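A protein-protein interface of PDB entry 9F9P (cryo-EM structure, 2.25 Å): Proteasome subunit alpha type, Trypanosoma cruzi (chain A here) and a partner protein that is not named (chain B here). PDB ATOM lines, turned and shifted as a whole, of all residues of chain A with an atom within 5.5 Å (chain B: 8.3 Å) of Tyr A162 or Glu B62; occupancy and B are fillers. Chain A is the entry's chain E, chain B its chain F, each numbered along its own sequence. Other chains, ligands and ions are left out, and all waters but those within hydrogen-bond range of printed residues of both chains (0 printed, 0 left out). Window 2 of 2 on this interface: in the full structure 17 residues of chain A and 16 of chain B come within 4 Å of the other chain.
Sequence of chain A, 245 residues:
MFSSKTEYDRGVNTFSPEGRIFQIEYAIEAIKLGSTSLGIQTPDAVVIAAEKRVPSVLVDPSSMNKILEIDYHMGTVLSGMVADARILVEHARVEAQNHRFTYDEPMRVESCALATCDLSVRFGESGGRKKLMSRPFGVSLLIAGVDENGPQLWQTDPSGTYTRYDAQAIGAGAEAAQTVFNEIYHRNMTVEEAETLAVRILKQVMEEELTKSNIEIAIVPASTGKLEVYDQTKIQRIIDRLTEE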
ATOM      1  N   GLU A 110      23.762 -14.129 -29.838  1.00  0.00           N
ATOM      2  CA  GLU A 110      23.497 -13.689 -28.481  1.00  0.00           C
ATOM      3  C   GLU A 110      22.013 -13.420 -28.227  1.00  0.00           C
ATOM      4  O   GLU A 110      21.547 -13.692 -27.130  1.00  0.00           O
ATOM      5  CB  GLU A 110      24.342 -12.451 -28.189  1.00  0.00           C
ATOM      6  CG  GLU A 110      24.130 -11.826 -26.815  1.00  0.00           C
ATOM      7  CD  GLU A 110      25.039 -10.624 -26.524  1.00  0.00           C
ATOM      8  OE1 GLU A 110      25.998 -10.382 -27.317  1.00  0.00           O
ATOM      9  OE2 GLU A 110      24.791  -9.910 -25.517  1.00  0.00           O
ATOM     10  N   ALA A 113      20.371 -16.823 -27.705  1.00  0.00           N
ATOM     11  CA  ALA A 113      20.680 -17.323 -26.371  1.00  0.00           C
ATOM     12  C   ALA A 113      19.775 -16.684 -25.319  1.00  0.00           C
ATOM     13  O   ALA A 113      19.211 -17.351 -24.467  1.00  0.00           O
ATOM     14  CB  ALA A 113      22.139 -17.077 -26.064  1.00  0.00           C
ATOM     15  N   LEU A 114      19.617 -15.374 -25.408  1.00  0.00           N
ATOM     16  CA  LEU A 114      18.771 -14.613 -24.514  1.00  0.00           C
ATOM     17  C   LEU A 114      17.319 -15.080 -24.587  1.00  0.00           C
ATOM     18  O   LEU A 114      16.687 -15.240 -23.557  1.00  0.00           O
ATOM     19  CB  LEU A 114      18.922 -13.131 -24.867  1.00  0.00           C
ATOM     20  CG  LEU A 114      17.940 -12.179 -24.177  1.00  0.00           C
ATOM     21  CD1 LEU A 114      18.194 -12.161 -22.679  1.00  0.00           C
ATOM     22  CD2 LEU A 114      18.024 -10.763 -24.739  1.00  0.00           C
ATOM     23  N   CYS A 117      16.710 -18.399 -22.683  1.00  0.00           N
ATOM     24  CA  CYS A 117      16.743 -18.214 -21.237  1.00  0.00           C
ATOM     25  C   CYS A 117      15.497 -17.561 -20.644  1.00  0.00           C
ATOM     26  O   CYS A 117      15.193 -17.754 -19.469  1.00  0.00           O
ATOM     27  CB  CYS A 117      17.939 -17.369 -20.866  1.00  0.00           C
ATOM     28  SG  CYS A 117      19.404 -18.386 -21.073  1.00  0.00           S
ATOM     29  N   TRP A 154      27.934 -19.731 -27.098  1.00  0.00           N
ATOM     30  CA  TRP A 154      27.264 -19.331 -25.865  1.00  0.00           C
ATOM     31  C   TRP A 154      26.746 -20.532 -25.091  1.00  0.00           C
ATOM     32  O   TRP A 154      26.305 -21.474 -25.705  1.00  0.00           O
ATOM     33  CB  TRP A 154      26.113 -18.388 -26.163  1.00  0.00           C
ATOM     34  CG  TRP A 154      26.541 -17.106 -26.787  1.00  0.00           C
ATOM     35  CD1 TRP A 154      26.925 -16.885 -28.079  1.00  0.00           C
ATOM     36  CD2 TRP A 154      26.634 -15.852 -26.116  1.00  0.00           C
ATOM     37  NE1 TRP A 154      27.268 -15.570 -28.249  1.00  0.00           N
ATOM     38  CE2 TRP A 154      27.105 -14.916 -27.063  1.00  0.00           C
ATOM     39  CE3 TRP A 154      26.413 -15.452 -24.799  1.00  0.00           C
ATOM     40  CZ2 TRP A 154      27.325 -13.586 -26.737  1.00  0.00           C
ATOM     41  CZ3 TRP A 154      26.616 -14.126 -24.474  1.00  0.00           C
ATOM     42  CH2 TRP A 154      27.106 -13.215 -25.421  1.00  0.00           C
ATOM     43  N   GLN A 155      26.706 -20.452 -23.755  1.00  0.00           N
ATOM     44  CA  GLN A 155      26.109 -21.504 -22.948  1.00  0.00           C
ATOM     45  C   GLN A 155      24.868 -20.998 -22.217  1.00  0.00           C
ATOM     46  O   GLN A 155      24.890 -19.909 -21.687  1.00  0.00           O
ATOM     47  CB  GLN A 155      27.112 -22.042 -21.941  1.00  0.00           C
ATOM     48  CG  GLN A 155      26.586 -23.283 -21.221  1.00  0.00           C
ATOM     49  CD  GLN A 155      27.323 -23.573 -19.944  1.00  0.00           C
ATOM     50  OE1 GLN A 155      26.993 -23.082 -18.869  1.00  0.00           O
ATOM     51  NE2 GLN A 155      28.396 -24.322 -20.072  1.00  0.00           N
ATOM     52  N   THR A 156      23.766 -21.766 -22.224  1.00  0.00           N
ATOM     53  CA  THR A 156      22.577 -21.469 -21.423  1.00  0.00           C
ATOM     54  C   THR A 156      22.479 -22.523 -20.331  1.00  0.00           C
ATOM     55  O   THR A 156      23.018 -23.590 -20.523  1.00  0.00           O
ATOM     56  CB  THR A 156      21.274 -21.449 -22.235  1.00  0.00           C
ATOM     57  OG1 THR A 156      20.969 -22.751 -22.740  1.00  0.00           O
ATOM     58  CG2 THR A 156      21.326 -20.512 -23.421  1.00  0.00           C
ATOM     59  N   GLY A 160      18.712 -19.704 -16.059  1.00  0.00           N
ATOM     60  CA  GLY A 160      18.510 -18.644 -17.038  1.00  0.00           C
ATOM     61  C   GLY A 160      19.688 -17.661 -17.173  1.00  0.00           C
ATOM     62  O   GLY A 160      19.482 -16.490 -17.490  1.00  0.00           O
ATOM     63  N   THR A 161      20.909 -18.110 -16.907  1.00  0.00           N
ATOM     64  CA  THR A 161      22.063 -17.288 -17.208  1.00  0.00           C
ATOM     65  C   THR A 161      22.710 -17.761 -18.503  1.00  0.00           C
ATOM     66  O   THR A 161      22.762 -18.956 -18.770  1.00  0.00           O
ATOM     67  CB  THR A 161      23.102 -17.227 -16.078  1.00  0.00           C
ATOM     68  OG1 THR A 161      24.368 -17.557 -16.652  1.00  0.00           O
ATOM     69  CG2 THR A 161      22.805 -18.159 -14.929  1.00  0.00           C
ATOM     70  N   TYR A 162      23.208 -16.800 -19.294  1.00  0.00           N
ATOM     71  CA  TYR A 162      23.893 -17.124 -20.523  1.00  0.00           C
ATOM     72  C   TYR A 162      25.256 -16.457 -20.510  1.00  0.00           C
ATOM     73  O   TYR A 162      25.405 -15.309 -20.122  1.00  0.00           O
ATOM     74  CB  TYR A 162      23.020 -16.795 -21.739  1.00  0.00           C
ATOM     75  CG  TYR A 162      22.656 -15.345 -21.918  1.00  0.00           C
ATOM     76  CD1 TYR A 162      23.396 -14.539 -22.767  1.00  0.00           C
ATOM     77  CD2 TYR A 162      21.534 -14.785 -21.313  1.00  0.00           C
ATOM     78  CE1 TYR A 162      23.091 -13.200 -22.940  1.00  0.00           C
ATOM     79  CE2 TYR A 162      21.194 -13.453 -21.510  1.00  0.00           C
ATOM     80  CZ  TYR A 162      22.002 -12.649 -22.298  1.00  0.00           C
ATOM     81  OH  TYR A 162      21.746 -11.324 -22.559  1.00  0.00           O
ATOM     82  N   THR A 163      26.240 -17.170 -21.011  1.00  0.00           N
ATOM     83  CA  THR A 163      27.621 -16.760 -20.901  1.00  0.00           C
ATOM     84  C   THR A 163      28.373 -17.097 -22.180  1.00  0.00           C
ATOM     85  O   THR A 163      28.203 -18.201 -22.655  1.00  0.00           O
ATOM     86  CB  THR A 163      28.261 -17.529 -19.746  1.00  0.00           C
ATOM     87  OG1 THR A 163      27.494 -17.191 -18.597  1.00  0.00           O
ATOM     88  CG2 THR A 163      29.718 -17.190 -19.555  1.00  0.00           C
ATOM     89  N   ARG A 164      29.249 -16.202 -22.663  1.00  0.00           N
ATOM     90  CA  ARG A 164      30.106 -16.478 -23.814  1.00  0.00           C
ATOM     91  C   ARG A 164      31.400 -17.173 -23.401  1.00  0.00           C
ATOM     92  O   ARG A 164      31.960 -16.862 -22.371  1.00  0.00           O
ATOM     93  CB  ARG A 164      30.474 -15.199 -24.553  1.00  0.00           C
ATOM     94  CG  ARG A 164      31.253 -15.454 -25.835  1.00  0.00           C
ATOM     95  CD  ARG A 164      31.460 -14.233 -26.704  1.00  0.00           C
ATOM     96  NE  ARG A 164      32.296 -14.567 -27.844  1.00  0.00           N
ATOM     97  CZ  ARG A 164      32.615 -13.724 -28.820  1.00  0.00           C
ATOM     98  NH1 ARG A 164      32.192 -12.471 -28.775  1.00  0.00           N
ATOM     99  NH2 ARG A 164      33.326 -14.150 -29.853  1.00  0.00           N
ATOM    100  N   SER B  33      28.712 -10.628  -7.113  1.00  0.00           N
ATOM    101  CA  SER B  33      30.003  -9.976  -7.283  1.00  0.00           C
ATOM    102  C   SER B  33      29.856  -8.489  -6.979  1.00  0.00           C
ATOM    103  O   SER B  33      28.776  -7.949  -7.133  1.00  0.00           O
ATOM    104  CB  SER B  33      30.564 -10.216  -8.669  1.00  0.00           C
ATOM    105  OG  SER B  33      29.544 -10.018  -9.640  1.00  0.00           O
ATOM    106  N   ALA B  48      31.747  -1.949 -11.431  1.00  0.00           N
ATOM    107  CA  ALA B  48      31.368  -3.326 -11.196  1.00  0.00           C
ATOM    108  C   ALA B  48      32.428  -4.279 -11.733  1.00  0.00           C
ATOM    109  O   ALA B  48      32.970  -4.078 -12.815  1.00  0.00           O
ATOM    110  CB  ALA B  48      30.060  -3.607 -11.885  1.00  0.00           C
ATOM    111  N   LEU B  49      32.585  -5.390 -11.008  1.00  0.00           N
ATOM    112  CA  LEU B  49      33.495  -6.476 -11.327  1.00  0.00           C
ATOM    113  C   LEU B  49      32.814  -7.545 -12.192  1.00  0.00           C
ATOM    114  O   LEU B  49      32.100  -8.388 -11.661  1.00  0.00           O
ATOM    115  CB  LEU B  49      33.916  -7.015  -9.962  1.00  0.00           C
ATOM    116  CG  LEU B  49      35.225  -7.788  -9.911  1.00  0.00           C
ATOM    117  CD1 LEU B  49      36.324  -7.031 -10.650  1.00  0.00           C
ATOM    118  CD2 LEU B  49      35.612  -8.032  -8.456  1.00  0.00           C
ATOM    119  N   LYS B  50      33.095  -7.539 -13.513  1.00  0.00           N
ATOM    120  CA  LYS B  50      32.392  -8.318 -14.532  1.00  0.00           C
ATOM    121  C   LYS B  50      33.241  -9.417 -15.217  1.00  0.00           C
ATOM    122  O   LYS B  50      32.827  -9.951 -16.255  1.00  0.00           O
ATOM    123  CB  LYS B  50      31.951  -7.383 -15.665  1.00  0.00           C
ATOM    124  CG  LYS B  50      33.032  -7.026 -16.694  1.00  0.00           C
ATOM    125  CD  LYS B  50      32.515  -6.664 -18.083  1.00  0.00           C
ATOM    126  CE  LYS B  50      33.195  -5.456 -18.712  1.00  0.00           C
ATOM    127  NZ  LYS B  50      34.406  -5.796 -19.497  1.00  0.00           N
ATOM    128  N   ARG B  51      34.434  -9.737 -14.676  1.00  0.00           N
ATOM    129  CA  ARG B  51      35.412 -10.691 -15.221  1.00  0.00           C
ATOM    130  C   ARG B  51      35.195 -11.013 -16.711  1.00  0.00           C
ATOM    131  O   ARG B  51      36.237 -11.175 -17.421  1.00  0.00           O
ATOM    132  CB  ARG B  51      35.444 -11.954 -14.350  1.00  0.00           C
ATOM    133  CG  ARG B  51      34.404 -13.014 -14.696  1.00  0.00           C
ATOM    134  CD  ARG B  51      33.936 -13.837 -13.501  1.00  0.00           C
ATOM    135  NE  ARG B  51      34.139 -15.273 -13.685  1.00  0.00           N
ATOM    136  CZ  ARG B  51      33.485 -16.045 -14.550  1.00  0.00           C
ATOM    137  NH1 ARG B  51      33.719 -17.348 -14.595  1.00  0.00           N
ATOM    138  NH2 ARG B  51      32.577 -15.517 -15.354  1.00  0.00           N
ATOM    139  N   SER B  59      34.497 -14.693 -21.648  1.00  0.00           N
ATOM    140  CA  SER B  59      33.733 -15.183 -20.469  1.00  0.00           C
ATOM    141  C   SER B  59      33.179 -13.961 -19.718  1.00  0.00           C
ATOM    142  O   SER B  59      33.391 -13.776 -18.519  1.00  0.00           O
ATOM    143  CB  SER B  59      34.578 -16.147 -19.620  1.00  0.00           C
ATOM    144  OG  SER B  59      35.008 -17.288 -20.368  1.00  0.00           O
ATOM    145  N   TYR B  60      32.443 -13.130 -20.473  1.00  0.00           N
ATOM    146  CA  TYR B  60      31.934 -11.833 -20.037  1.00  0.00           C
ATOM    147  C   TYR B  60      30.526 -12.011 -19.450  1.00  0.00           C
ATOM    148  O   TYR B  60      29.678 -12.626 -20.099  1.00  0.00           O
ATOM    149  CB  TYR B  60      32.008 -10.876 -21.242  1.00  0.00           C
ATOM    150  CG  TYR B  60      30.831  -9.954 -21.472  1.00  0.00           C
ATOM    151  CD1 TYR B  60      30.723  -8.740 -20.809  1.00  0.00           C
ATOM    152  CD2 TYR B  60      29.821 -10.290 -22.366  1.00  0.00           C
ATOM    153  CE1 TYR B  60      29.647  -7.889 -21.020  1.00  0.00           C
ATOM    154  CE2 TYR B  60      28.735  -9.453 -22.584  1.00  0.00           C
ATOM    155  CZ  TYR B  60      28.648  -8.247 -21.909  1.00  0.00           C
ATOM    156  OH  TYR B  60      27.583  -7.400 -22.109  1.00  0.00           O
ATOM    157  N   GLN B  61      30.278 -11.484 -18.232  1.00  0.00           N
ATOM    158  CA  GLN B  61      28.971 -11.612 -17.586  1.00  0.00           C
ATOM    159  C   GLN B  61      28.363 -10.228 -17.331  1.00  0.00           C
ATOM    160  O   GLN B  61      28.925  -9.432 -16.584  1.00  0.00           O
ATOM    161  CB  GLN B  61      29.086 -12.419 -16.286  1.00  0.00           C
ATOM    162  CG  GLN B  61      28.145 -13.629 -16.225  1.00  0.00           C
ATOM    163  CD  GLN B  61      26.807 -13.378 -15.567  1.00  0.00           C
ATOM    164  OE1 GLN B  61      26.668 -13.448 -14.345  1.00  0.00           O
ATOM    165  NE2 GLN B  61      25.789 -13.140 -16.379  1.00  0.00           N
ATOM    166  N   GLU B  62      27.177  -9.988 -17.920  1.00  0.00           N
ATOM    167  CA  GLU B  62      26.525  -8.680 -17.967  1.00  0.00           C
ATOM    168  C   GLU B  62      25.987  -8.272 -16.592  1.00  0.00           C
ATOM    169  O   GLU B  62      25.140  -8.956 -16.017  1.00  0.00           O
ATOM    170  CB  GLU B  62      25.357  -8.737 -18.961  1.00  0.00           C
ATOM    171  CG  GLU B  62      25.012  -7.404 -19.621  1.00  0.00           C
ATOM    172  CD  GLU B  62      23.644  -7.346 -20.293  1.00  0.00           C
ATOM    173  OE1 GLU B  62      23.251  -8.350 -20.931  1.00  0.00           O
ATOM    174  OE2 GLU B  62      22.973  -6.291 -20.191  1.00  0.00           O
ATOM    175  N   LYS B  63      26.440  -7.123 -16.095  1.00  0.00           N
ATOM    176  CA  LYS B  63      26.099  -6.677 -14.759  1.00  0.00           C
ATOM    177  C   LYS B  63      25.447  -5.278 -14.728  1.00  0.00           C
ATOM    178  O   LYS B  63      24.874  -4.896 -13.724  1.00  0.00           O
ATOM    179  CB  LYS B  63      27.406  -6.725 -13.977  1.00  0.00           C
ATOM    180  CG  LYS B  63      27.272  -6.630 -12.474  1.00  0.00           C
ATOM    181  CD  LYS B  63      28.324  -7.436 -11.737  1.00  0.00           C
ATOM    182  CE  LYS B  63      28.406  -7.078 -10.262  1.00  0.00           C
ATOM    183  NZ  LYS B  63      27.372  -7.778  -9.460  1.00  0.00           N
ATOM    184  N   VAL B  64      25.561  -4.501 -15.813  1.00  0.00           N
ATOM    185  CA  VAL B  64      25.050  -3.151 -15.912  1.00  0.00           C
ATOM    186  C   VAL B  64      24.101  -3.031 -17.093  1.00  0.00           C
ATOM    187  O   VAL B  64      24.374  -3.586 -18.145  1.00  0.00           O
ATOM    188  CB  VAL B  64      26.189  -2.144 -16.069  1.00  0.00           C
ATOM    189  CG1 VAL B  64      25.636  -0.735 -16.201  1.00  0.00           C
ATOM    190  CG2 VAL B  64      27.148  -2.226 -14.894  1.00  0.00           C
ATOM    191  N   PHE B  65      22.993  -2.317 -16.882  1.00  0.00           N
ATOM    192  CA  PHE B  65      21.893  -2.203 -17.814  1.00  0.00           C
ATOM    193  C   PHE B  65      21.365  -0.778 -17.880  1.00  0.00           C
ATOM    194  O   PHE B  65      21.058  -0.203 -16.856  1.00  0.00           O
ATOM    195  CB  PHE B  65      20.693  -2.998 -17.331  1.00  0.00           C
ATOM    196  CG  PHE B  65      20.878  -4.481 -17.230  1.00  0.00           C
ATOM    197  CD1 PHE B  65      20.183  -5.333 -18.080  1.00  0.00           C
ATOM    198  CD2 PHE B  65      21.662  -5.035 -16.232  1.00  0.00           C
ATOM    199  CE1 PHE B  65      20.320  -6.713 -17.975  1.00  0.00           C
ATOM    200  CE2 PHE B  65      21.809  -6.415 -16.135  1.00  0.00           C
ATOM    201  CZ  PHE B  65      21.135  -7.249 -17.001  1.00  0.00           C
ATOM    202  N   LYS B  66      21.166  -0.251 -19.084  1.00  0.00           N
ATOM    203  CA  LYS B  66      20.507   1.023 -19.317  1.00  0.00           C
ATOM    204  C   LYS B  66      18.986   0.907 -19.158  1.00  0.00           C
ATOM    205  O   LYS B  66      18.388  -0.036 -19.656  1.00  0.00           O
ATOM    206  CB  LYS B  66      20.880   1.430 -20.737  1.00  0.00           C
ATOM    207  CG  LYS B  66      20.366   2.774 -21.236  1.00  0.00           C
ATOM    208  CD  LYS B  66      21.133   3.263 -22.467  1.00  0.00           C
ATOM    209  CE  LYS B  66      20.511   4.453 -23.175  1.00  0.00           C
ATOM    210  NZ  LYS B  66      19.100   4.152 -23.538  1.00  0.00           N
ATOM    211  N   MET B  73      21.272   0.902 -14.091  1.00  0.00           N
ATOM    212  CA  MET B  73      21.565   0.211 -12.836  1.00  0.00           C
ATOM    213  C   MET B  73      22.649  -0.865 -12.938  1.00  0.00           C
ATOM    214  O   MET B  73      22.867  -1.416 -14.002  1.00  0.00           O
ATOM    215  CB  MET B  73      20.295  -0.487 -12.352  1.00  0.00           C
ATOM    216  CG  MET B  73      19.830  -1.591 -13.258  1.00  0.00           C
ATOM    217  SD  MET B  73      18.182  -2.186 -12.673  1.00  0.00           S
ATOM    218  CE  MET B  73      18.116  -3.768 -13.522  1.00  0.00           C
ATOM    219  N   ALA B  74      23.232  -1.225 -11.785  1.00  0.00           N
ATOM    220  CA  ALA B  74      24.015  -2.440 -11.613  1.00  0.00           C
ATOM    221  C   ALA B  74      23.273  -3.471 -10.760  1.00  0.00           C
ATOM    222  O   ALA B  74      22.574  -3.095  -9.835  1.00  0.00           O
ATOM    223  CB  ALA B  74      25.302  -2.103 -10.941  1.00  0.00           C
ATOM    224  N   ILE B  75      23.433  -4.767 -11.042  1.00  0.00           N
ATOM    225  CA  ILE B  75      22.797  -5.780 -10.219  1.00  0.00           C
ATOM    226  C   ILE B  75      23.804  -6.661  -9.477  1.00  0.00           C
ATOM    227  O   ILE B  75      24.973  -6.662  -9.841  1.00  0.00           O
ATOM    228  CB  ILE B  75      21.887  -6.646 -11.084  1.00  0.00           C
ATOM    229  CG1 ILE B  75      22.704  -7.587 -11.947  1.00  0.00           C
ATOM    230  CG2 ILE B  75      20.933  -5.783 -11.898  1.00  0.00           C
ATOM    231  CD1 ILE B  75      21.823  -8.385 -12.894  1.00  0.00           C
ATOM    232  N   ALA B  76      23.325  -7.353  -8.420  1.00  0.00           N
ATOM    233  CA  ALA B  76      24.042  -8.412  -7.714  1.00  0.00           C
ATOM    234  C   ALA B  76      23.071  -9.487  -7.226  1.00  0.00           C
ATOM    235  O   ALA B  76      22.074  -9.145  -6.606  1.00  0.00           O
ATOM    236  CB  ALA B  76      24.804  -7.871  -6.544  1.00  0.00           C
ATOM    237  N   GLY B  77      23.364 -10.769  -7.499  1.00  0.00           N
ATOM    238  CA  GLY B  77      22.504 -11.885  -7.132  1.00  0.00           C
ATOM    239  C   GLY B  77      21.993 -12.627  -8.361  1.00  0.00           C
ATOM    240  O   GLY B  77      22.699 -12.741  -9.344  1.00  0.00           O
ATOM    241  N   VAL B  79      20.724 -13.251 -11.786  1.00  0.00           N
ATOM    242  CA  VAL B  79      20.609 -12.502 -13.027  1.00  0.00           C
ATOM    243  C   VAL B  79      19.224 -12.615 -13.661  1.00  0.00           C
ATOM    244  O   VAL B  79      18.743 -11.641 -14.231  1.00  0.00           O
ATOM    245  CB  VAL B  79      21.682 -12.915 -14.042  1.00  0.00           C
ATOM    246  CG1 VAL B  79      21.723 -11.922 -15.194  1.00  0.00           C
ATOM    247  CG2 VAL B  79      23.052 -13.022 -13.380  1.00  0.00           C
ATOM    248  N   ALA B  80      18.556 -13.762 -13.618  1.00  0.00           N
ATOM    249  CA  ALA B  80      17.285 -13.813 -14.317  1.00  0.00           C
ATOM    250  C   ALA B  80      16.241 -12.923 -13.627  1.00  0.00           C
ATOM    251  O   ALA B  80      15.349 -12.407 -14.320  1.00  0.00           O
ATOM    252  CB  ALA B  80      16.755 -15.214 -14.499  1.00  0.00           C
ATOM    253  N   GLY B  82      17.192 -10.001 -12.054  1.00  0.00           N
ATOM    254  CA  GLY B  82      17.696  -8.741 -12.578  1.00  0.00           C
ATOM    255  C   GLY B  82      17.013  -8.342 -13.887  1.00  0.00           C
ATOM    256  O   GLY B  82      16.493  -7.229 -13.972  1.00  0.00           O
ATOM    257  N   ARG B  83      16.983  -9.270 -14.857  1.00  0.00           N
ATOM    258  CA  ARG B  83      16.432  -9.023 -16.178  1.00  0.00           C
ATOM    259  C   ARG B  83      14.931  -8.759 -16.129  1.00  0.00           C
ATOM    260  O   ARG B  83      14.431  -7.939 -16.894  1.00  0.00           O
ATOM    261  CB  ARG B  83      16.630 -10.208 -17.141  1.00  0.00           C
ATOM    262  CG  ARG B  83      18.055 -10.401 -17.644  1.00  0.00           C
ATOM    263  CD  ARG B  83      18.032 -11.117 -18.989  1.00  0.00           C
ATOM    264  NE  ARG B  83      17.519 -12.476 -18.886  1.00  0.00           N
ATOM    265  CZ  ARG B  83      18.226 -13.523 -18.444  1.00  0.00           C
ATOM    266  NH1 ARG B  83      17.619 -14.692 -18.290  1.00  0.00           N
ATOM    267  NH2 ARG B  83      19.513 -13.395 -18.148  1.00  0.00           N
ATOM    268  N   ALA B  86      14.630  -5.160 -14.882  1.00  0.00           N
ATOM    269  CA  ALA B  86      15.002  -4.287 -15.996  1.00  0.00           C
ATOM    270  C   ALA B  86      13.883  -4.147 -17.018  1.00  0.00           C
ATOM    271  O   ALA B  86      13.571  -3.034 -17.389  1.00  0.00           O
ATOM    272  CB  ALA B  86      16.230  -4.762 -16.658  1.00  0.00           C
ATOM    273  N   ARG B  90      12.079  -0.453 -17.653  1.00  0.00           N
ATOM    274  CA  ARG B  90      12.117   0.038 -19.014  1.00  0.00           C
ATOM    275  C   ARG B  90      10.706   0.392 -19.478  1.00  0.00           C
ATOM    276  O   ARG B  90      10.468   1.473 -19.990  1.00  0.00           O
ATOM    277  CB  ARG B  90      12.771  -0.998 -19.932  1.00  0.00           C
ATOM    278  CG  ARG B  90      14.295  -0.947 -19.864  1.00  0.00           C
ATOM    279  CD  ARG B  90      14.912  -2.251 -20.335  1.00  0.00           C
ATOM    280  NE  ARG B  90      16.340  -2.128 -20.382  1.00  0.00           N
ATOM    281  CZ  ARG B  90      17.153  -3.106 -20.761  1.00  0.00           C
ATOM    282  NH1 ARG B  90      16.651  -4.278 -21.116  1.00  0.00           N
ATOM    283  NH2 ARG B  90      18.455  -2.854 -20.784  1.00  0.00           N
ATOM    284  N   THR B 212      33.668  -2.739 -15.377  1.00  0.00           N
ATOM    285  CA  THR B 212      32.740  -1.848 -16.051  1.00  0.00           C
ATOM    286  C   THR B 212      32.747  -0.497 -15.328  1.00  0.00           C
ATOM    287  O   THR B 212      32.853  -0.444 -14.111  1.00  0.00           O
ATOM    288  CB  THR B 212      31.316  -2.442 -16.038  1.00  0.00           C
ATOM    289  OG1 THR B 212      31.221  -3.676 -16.752  1.00  0.00           O
ATOM    290  CG2 THR B 212      30.275  -1.505 -16.628  1.00  0.00           C
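The backbone carbonyl oxygen of Ala A113 sits at hydrogen-bond distance from the side-chain sulfur of Cys A117, 3.6 Å away.
Among the printed residues, pairs that only touch across the chains: Leu A114 with Arg B83, Cys A117 with Arg B83, Tyr A162 with Glu B62 and Tyr A162 with Arg B83.
Among the printed residues, 6 pairs touch across the chains.
The guanidinium group (NH1) of Arg B83 lies within hydrogen-bond range of the backbone carbonyl oxygen (O) of Gly A160, at 2.7 Å. The backbone carbonyl oxygen (O) of Arg A164 sits close to the backbone NH (N) of Ser B59.
Tyr A162 touches two residues of chain B. Glu B62 touches just one residue of chain A: Tyr A162 (3.7 Å). Printed residues of chain A within 4 Å of Arg B83: Leu A114, Cys A117, Gly A160 and Tyr A162. Of the printed residues of chain B, Arg A164 touches Ser B59. Of the printed residues of chain B, Gly A160 touches Arg B83. Lys B63 touches none of the printed residues of chain A. Gln B61 touches none of the printed residues of chain A. The nearest printed residue of chain A that does not touch Arg B83 is Thr A161 (4.7 Å).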
